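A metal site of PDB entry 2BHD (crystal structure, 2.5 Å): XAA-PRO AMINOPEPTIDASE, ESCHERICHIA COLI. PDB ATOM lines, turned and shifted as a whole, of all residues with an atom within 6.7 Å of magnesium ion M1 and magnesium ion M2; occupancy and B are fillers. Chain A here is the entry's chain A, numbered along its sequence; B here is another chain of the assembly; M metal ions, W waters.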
ATOM      1  N   TYR A 229     -15.641  -0.071  10.805  1.00  0.00           N
ATOM      2  CA  TYR A 229     -15.833  -0.258   9.364  1.00  0.00           C
ATOM      3  C   TYR A 229     -15.127   0.874   8.620  1.00  0.00           C
ATOM      4  O   TYR A 229     -14.800   1.889   9.206  1.00  0.00           O
ATOM      5  CB  TYR A 229     -17.337  -0.278   8.980  1.00  0.00           C
ATOM      6  CG  TYR A 229     -18.086   0.935   9.463  1.00  0.00           C
ATOM      7  CD1 TYR A 229     -18.574   0.992  10.753  1.00  0.00           C
ATOM      8  CD2 TYR A 229     -18.258   2.046   8.647  1.00  0.00           C
ATOM      9  CE1 TYR A 229     -19.248   2.107  11.229  1.00  0.00           C
ATOM     10  CE2 TYR A 229     -18.940   3.175   9.108  1.00  0.00           C
ATOM     11  CZ  TYR A 229     -19.424   3.202  10.394  1.00  0.00           C
ATOM     12  OH  TYR A 229     -20.103   4.298  10.881  1.00  0.00           O
ATOM     13  N   ILE A 232     -16.604   6.543   5.641  1.00  0.00           N
ATOM     14  CA  ILE A 232     -17.232   7.108   4.450  1.00  0.00           C
ATOM     15  C   ILE A 232     -17.247   8.626   4.578  1.00  0.00           C
ATOM     16  O   ILE A 232     -17.840   9.167   5.520  1.00  0.00           O
ATOM     17  CB  ILE A 232     -18.687   6.577   4.305  1.00  0.00           C
ATOM     18  CG1 ILE A 232     -18.682   5.064   3.989  1.00  0.00           C
ATOM     19  CG2 ILE A 232     -19.479   7.356   3.245  1.00  0.00           C
ATOM     20  CD1 ILE A 232     -19.942   4.358   4.427  1.00  0.00           C
ATOM     21  N   ASP A 260     -20.060   8.846   7.363  1.00  0.00           N
ATOM     22  CA  ASP A 260     -20.479   7.625   8.065  1.00  0.00           C
ATOM     23  C   ASP A 260     -19.208   6.974   8.639  1.00  0.00           C
ATOM     24  O   ASP A 260     -18.349   6.443   7.900  1.00  0.00           O
ATOM     25  CB  ASP A 260     -21.241   6.663   7.132  1.00  0.00           C
ATOM     26  CG  ASP A 260     -22.065   5.587   7.890  1.00  0.00           C
ATOM     27  OD1 ASP A 260     -21.800   5.259   9.079  1.00  0.00           O
ATOM     28  OD2 ASP A 260     -23.027   5.051   7.283  1.00  0.00           O
ATOM     29  N   ALA A 261     -19.084   7.039   9.965  1.00  0.00           N
ATOM     30  CA  ALA A 261     -17.901   6.552  10.655  1.00  0.00           C
ATOM     31  C   ALA A 261     -18.225   6.075  12.048  1.00  0.00           C
ATOM     32  O   ALA A 261     -19.138   6.602  12.718  1.00  0.00           O
ATOM     33  CB  ALA A 261     -16.852   7.609  10.700  1.00  0.00           C
ATOM     34  N   ASP A 271     -21.556   3.615  15.311  1.00  0.00           N
ATOM     35  CA  ASP A 271     -21.930   3.768  13.899  1.00  0.00           C
ATOM     36  C   ASP A 271     -22.778   5.027  13.785  1.00  0.00           C
ATOM     37  O   ASP A 271     -23.968   4.998  14.070  1.00  0.00           O
ATOM     38  CB  ASP A 271     -22.695   2.532  13.398  1.00  0.00           C
ATOM     39  CG  ASP A 271     -23.176   2.666  11.951  1.00  0.00           C
ATOM     40  OD1 ASP A 271     -22.840   3.643  11.255  1.00  0.00           O
ATOM     41  OD2 ASP A 271     -23.920   1.762  11.493  1.00  0.00           O
ATOM     42  N   ILE A 272     -22.155   6.125  13.373  1.00  0.00           N
ATOM     43  CA  ILE A 272     -22.837   7.400  13.262  1.00  0.00           C
ATOM     44  C   ILE A 272     -22.709   7.953  11.837  1.00  0.00           C
ATOM     45  O   ILE A 272     -21.656   7.842  11.190  1.00  0.00           O
ATOM     46  CB  ILE A 272     -22.271   8.439  14.257  1.00  0.00           C
ATOM     47  CG1 ILE A 272     -22.606   8.046  15.691  1.00  0.00           C
ATOM     48  CG2 ILE A 272     -22.840   9.840  13.982  1.00  0.00           C
ATOM     49  CD1 ILE A 272     -22.081   9.030  16.701  1.00  0.00           C
ATOM     50  N   THR A 273     -23.783   8.558  11.356  1.00  0.00           N
ATOM     51  CA  THR A 273     -23.721   9.331  10.116  1.00  0.00           C
ATOM     52  C   THR A 273     -24.193  10.732  10.419  1.00  0.00           C
ATOM     53  O   THR A 273     -25.198  10.910  11.112  1.00  0.00           O
ATOM     54  CB  THR A 273     -24.569   8.750   8.977  1.00  0.00           C
ATOM     55  OG1 THR A 273     -24.312   7.349   8.823  1.00  0.00           O
ATOM     56  CG2 THR A 273     -24.243   9.466   7.659  1.00  0.00           C
ATOM     57  N   HIS A 354     -30.320  -1.439  11.412  1.00  0.00           N
ATOM     58  CA  HIS A 354     -29.731  -2.759  11.570  1.00  0.00           C
ATOM     59  C   HIS A 354     -29.301  -2.946  13.012  1.00  0.00           C
ATOM     60  O   HIS A 354     -29.054  -1.974  13.692  1.00  0.00           O
ATOM     61  CB  HIS A 354     -28.538  -2.971  10.628  1.00  0.00           C
ATOM     62  CG  HIS A 354     -27.467  -1.915  10.727  1.00  0.00           C
ATOM     63  ND1 HIS A 354     -26.486  -1.939  11.687  1.00  0.00           N
ATOM     64  CD2 HIS A 354     -27.222  -0.828   9.953  1.00  0.00           C
ATOM     65  CE1 HIS A 354     -25.682  -0.898  11.519  1.00  0.00           C
ATOM     66  NE2 HIS A 354     -26.112  -0.210  10.477  1.00  0.00           N
ATOM     67  N   LEU A 356     -26.815  -3.620  16.078  1.00  0.00           N
ATOM     68  CA  LEU A 356     -25.468  -3.132  16.330  1.00  0.00           C
ATOM     69  C   LEU A 356     -24.854  -3.865  17.525  1.00  0.00           C
ATOM     70  O   LEU A 356     -25.530  -4.091  18.542  1.00  0.00           O
ATOM     71  CB  LEU A 356     -25.523  -1.637  16.629  1.00  0.00           C
ATOM     72  CG  LEU A 356     -24.213  -0.877  16.783  1.00  0.00           C
ATOM     73  CD1 LEU A 356     -23.472  -0.814  15.459  1.00  0.00           C
ATOM     74  CD2 LEU A 356     -24.513   0.525  17.323  1.00  0.00           C
ATOM     75  N   VAL A 360     -20.727  -4.234  13.303  1.00  0.00           N
ATOM     76  CA  VAL A 360     -21.495  -3.050  13.002  1.00  0.00           C
ATOM     77  C   VAL A 360     -22.860  -3.445  12.399  1.00  0.00           C
ATOM     78  O   VAL A 360     -23.875  -2.895  12.787  1.00  0.00           O
ATOM     79  CB  VAL A 360     -20.723  -2.017  12.136  1.00  0.00           C
ATOM     80  CG1 VAL A 360     -20.365  -2.577  10.769  1.00  0.00           C
ATOM     81  CG2 VAL A 360     -21.548  -0.735  11.978  1.00  0.00           C
ATOM     82  N   HIS A 361     -22.872  -4.394  11.483  1.00  0.00           N
ATOM     83  CA  HIS A 361     -24.107  -5.028  11.020  1.00  0.00           C
ATOM     84  C   HIS A 361     -24.257  -6.295  11.832  1.00  0.00           C
ATOM     85  O   HIS A 361     -23.818  -7.370  11.409  1.00  0.00           O
ATOM     86  CB  HIS A 361     -24.059  -5.398   9.538  1.00  0.00           C
ATOM     87  CG  HIS A 361     -24.016  -4.222   8.622  1.00  0.00           C
ATOM     88  ND1 HIS A 361     -23.587  -4.317   7.313  1.00  0.00           N
ATOM     89  CD2 HIS A 361     -24.331  -2.920   8.815  1.00  0.00           C
ATOM     90  CE1 HIS A 361     -23.650  -3.127   6.748  1.00  0.00           C
ATOM     91  NE2 HIS A 361     -24.100  -2.260   7.632  1.00  0.00           N
ATOM     92  N   THR A 381     -29.397   0.720  14.891  1.00  0.00           N
ATOM     93  CA  THR A 381     -29.199   2.019  14.276  1.00  0.00           C
ATOM     94  C   THR A 381     -30.531   2.596  13.776  1.00  0.00           C
ATOM     95  O   THR A 381     -31.502   1.863  13.539  1.00  0.00           O
ATOM     96  CB  THR A 381     -28.206   1.962  13.118  1.00  0.00           C
ATOM     97  OG1 THR A 381     -28.723   1.129  12.069  1.00  0.00           O
ATOM     98  CG2 THR A 381     -26.863   1.412  13.605  1.00  0.00           C
ATOM     99  N   VAL A 382     -30.571   3.922  13.660  1.00  0.00           N
ATOM    100  CA  VAL A 382     -31.692   4.605  13.053  1.00  0.00           C
ATOM    101  C   VAL A 382     -31.077   5.545  12.027  1.00  0.00           C
ATOM    102  O   VAL A 382     -30.436   6.531  12.405  1.00  0.00           O
ATOM    103  CB  VAL A 382     -32.527   5.380  14.080  1.00  0.00           C
ATOM    104  CG1 VAL A 382     -33.813   5.893  13.435  1.00  0.00           C
ATOM    105  CG2 VAL A 382     -32.862   4.507  15.277  1.00  0.00           C
ATOM    106  N   GLU A 383     -31.253   5.237  10.752  1.00  0.00           N
ATOM    107  CA  GLU A 383     -30.498   5.899   9.710  1.00  0.00           C
ATOM    108  C   GLU A 383     -31.272   6.161   8.423  1.00  0.00           C
ATOM    109  O   GLU A 383     -30.926   5.623   7.374  1.00  0.00           O
ATOM    110  CB  GLU A 383     -29.233   5.106   9.412  1.00  0.00           C
ATOM    111  CG  GLU A 383     -29.427   3.658   9.015  1.00  0.00           C
ATOM    112  CD  GLU A 383     -28.103   2.973   8.755  1.00  0.00           C
ATOM    113  OE1 GLU A 383     -27.323   3.495   7.925  1.00  0.00           O
ATOM    114  OE2 GLU A 383     -27.809   1.941   9.407  1.00  0.00           O
ATOM    115  N   ARG A 404     -27.768  11.494   4.886  1.00  0.00           N
ATOM    116  CA  ARG A 404     -28.130  10.470   5.847  1.00  0.00           C
ATOM    117  C   ARG A 404     -27.799  10.999   7.228  1.00  0.00           C
ATOM    118  O   ARG A 404     -26.801  11.692   7.400  1.00  0.00           O
ATOM    119  CB  ARG A 404     -27.382   9.165   5.581  1.00  0.00           C
ATOM    120  CG  ARG A 404     -27.615   8.059   6.596  1.00  0.00           C
ATOM    121  CD  ARG A 404     -27.214   6.668   6.094  1.00  0.00           C
ATOM    122  NE  ARG A 404     -25.770   6.471   5.917  1.00  0.00           N
ATOM    123  CZ  ARG A 404     -25.123   6.444   4.753  1.00  0.00           C
ATOM    124  NH1 ARG A 404     -25.753   6.660   3.598  1.00  0.00           N
ATOM    125  NH2 ARG A 404     -23.820   6.226   4.714  1.00  0.00           N
ATOM    126  N   GLU A 406     -27.666   9.310  11.156  1.00  0.00           N
ATOM    127  CA  GLU A 406     -27.712   8.016  11.829  1.00  0.00           C
ATOM    128  C   GLU A 406     -27.334   8.149  13.308  1.00  0.00           C
ATOM    129  O   GLU A 406     -26.307   8.713  13.645  1.00  0.00           O
ATOM    130  CB  GLU A 406     -26.787   7.015  11.115  1.00  0.00           C
ATOM    131  CG  GLU A 406     -26.500   5.691  11.853  1.00  0.00           C
ATOM    132  CD  GLU A 406     -25.777   4.667  10.969  1.00  0.00           C
ATOM    133  OE1 GLU A 406     -24.930   5.082  10.120  1.00  0.00           O
ATOM    134  OE2 GLU A 406     -26.032   3.445  11.111  1.00  0.00           O
ATOM    135  N   ASP A 408     -27.390   5.703  17.103  1.00  0.00           N
ATOM    136  CA  ASP A 408     -27.387   4.355  17.679  1.00  0.00           C
ATOM    137  C   ASP A 408     -28.221   4.362  18.953  1.00  0.00           C
ATOM    138  O   ASP A 408     -28.072   5.251  19.801  1.00  0.00           O
ATOM    139  CB  ASP A 408     -25.955   3.920  18.039  1.00  0.00           C
ATOM    140  CG  ASP A 408     -24.992   4.021  16.856  1.00  0.00           C
ATOM    141  OD1 ASP A 408     -25.454   3.888  15.698  1.00  0.00           O
ATOM    142  OD2 ASP A 408     -23.790   4.232  17.102  1.00  0.00           O
ATOM    143  N   PRO B   2     -25.202   1.482   5.911  1.00  0.00           N
ATOM    144  CA  PRO B   2     -26.577   1.048   5.685  1.00  0.00           C
ATOM    145  C   PRO B   2     -26.673  -0.431   5.355  1.00  0.00           C
ATOM    146  O   PRO B   2     -25.719  -0.997   4.792  1.00  0.00           O
ATOM    147  CB  PRO B   2     -26.994   1.884   4.475  1.00  0.00           C
ATOM    148  CG  PRO B   2     -26.219   3.115   4.575  1.00  0.00           C
ATOM    149  CD  PRO B   2     -24.915   2.761   5.239  1.00  0.00           C
ATOM    150  N   LEU B   3     -27.793  -1.044   5.725  1.00  0.00           N
ATOM    151  CA  LEU B   3     -28.140  -2.428   5.369  1.00  0.00           C
ATOM    152  C   LEU B   3     -29.501  -2.407   4.655  1.00  0.00           C
ATOM    153  O   LEU B   3     -29.710  -3.068   3.634  1.00  0.00           O
ATOM    154  CB  LEU B   3     -28.191  -3.336   6.620  1.00  0.00           C
ATOM    155  CG  LEU B   3     -28.223  -4.877   6.467  1.00  0.00           C
ATOM    156  CD1 LEU B   3     -27.019  -5.428   5.724  1.00  0.00           C
ATOM    157  CD2 LEU B   3     -28.324  -5.549   7.817  1.00  0.00           C
ATOM    158  OXT LEU B   3     -30.430  -1.712   5.057  1.00  0.00           O
HETATM  159 MG    MG M   1     -23.527   3.762   9.383  1.00  0.00          MG
HETATM  160 MG    MG M   2     -25.531   1.811  10.160  1.00  0.00          MG
HETATM  161  O   HOH W   1     -24.702   2.591   8.514  1.00  0.00           O
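The backbone NH of Glu 406 is in hydrogen-bond range of the backbone carbonyl oxygen of Thr 273.
The backbone NH of Asp 271 is in hydrogen-bond range of the side-chain carboxylate of Asp 408, 2.9 Å away.
The backbone carbonyl oxygen (O) of His 354 lies within hydrogen-bond range of the backbone NH (N) of Thr 381 (3.0 Å).
A ring nitrogen (ND1) of His 354 sits close to the backbone carbonyl oxygen (O) of Val 360 (3.0 Å).
The backbone carbonyl oxygen (O) of Asp 260 sits at hydrogen-bond distance from the backbone NH (N) of Ile 232.
The side-chain carboxylate (OE2) of Glu 383 sits close to the side-chain hydroxyl (OG1) of Thr 381.
The side-chain hydroxyl (OG1) of Thr 273 is in hydrogen-bond range of the guanidinium group (NE) of Arg 404, at 3.4 Å.
N of Ala 261 lies close to OH of Tyr 229, 3.1 Å away.
Tyr 229 touches magnesium ion M1.
Thr 273 touches magnesium ion M1.
Five residues have an atom within 4 Å of magnesium ion M1: Tyr 229, Asp 260, Asp 271, Thr 273 and Glu 406.
The nearest printed residue that does not touch magnesium ion M1 is Glu 383 (4.1 Å).
Thr 381 touches magnesium ion M2 (CG2 to MG, 3.7 Å).
Five residues have an atom within 4 Å of magnesium ion M2: Asp 271, His 354, Thr 381, Glu 383 and Glu 406.
The nearest printed residue that does not touch magnesium ion M2 is Pro 2 of chain B (4.3 Å).
Magnesium ion M1 is bound by water W1 (1.9 Å), the side-chain carboxylate (OD1) of Asp 271 (2.0 Å), the side-chain carboxylate (OE1) of Glu 406 (2.1 Å), the side-chain carboxylate (OD1) of Asp 260 (2.3 Å) and the side-chain carboxylate (OD2) of Asp 260 (2.5 Å).
Magnesium ion M1 has five donor atoms within binding distance.
Magnesium ion M2 is bound by the side-chain carboxylate of Glu 406, water W1, the side-chain carboxylate of Asp 271, a ring nitrogen (NE2) of His 354 and the side-chain carboxylate of Glu 383.
Magnesium ion M2 has five donor atoms within binding distance.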
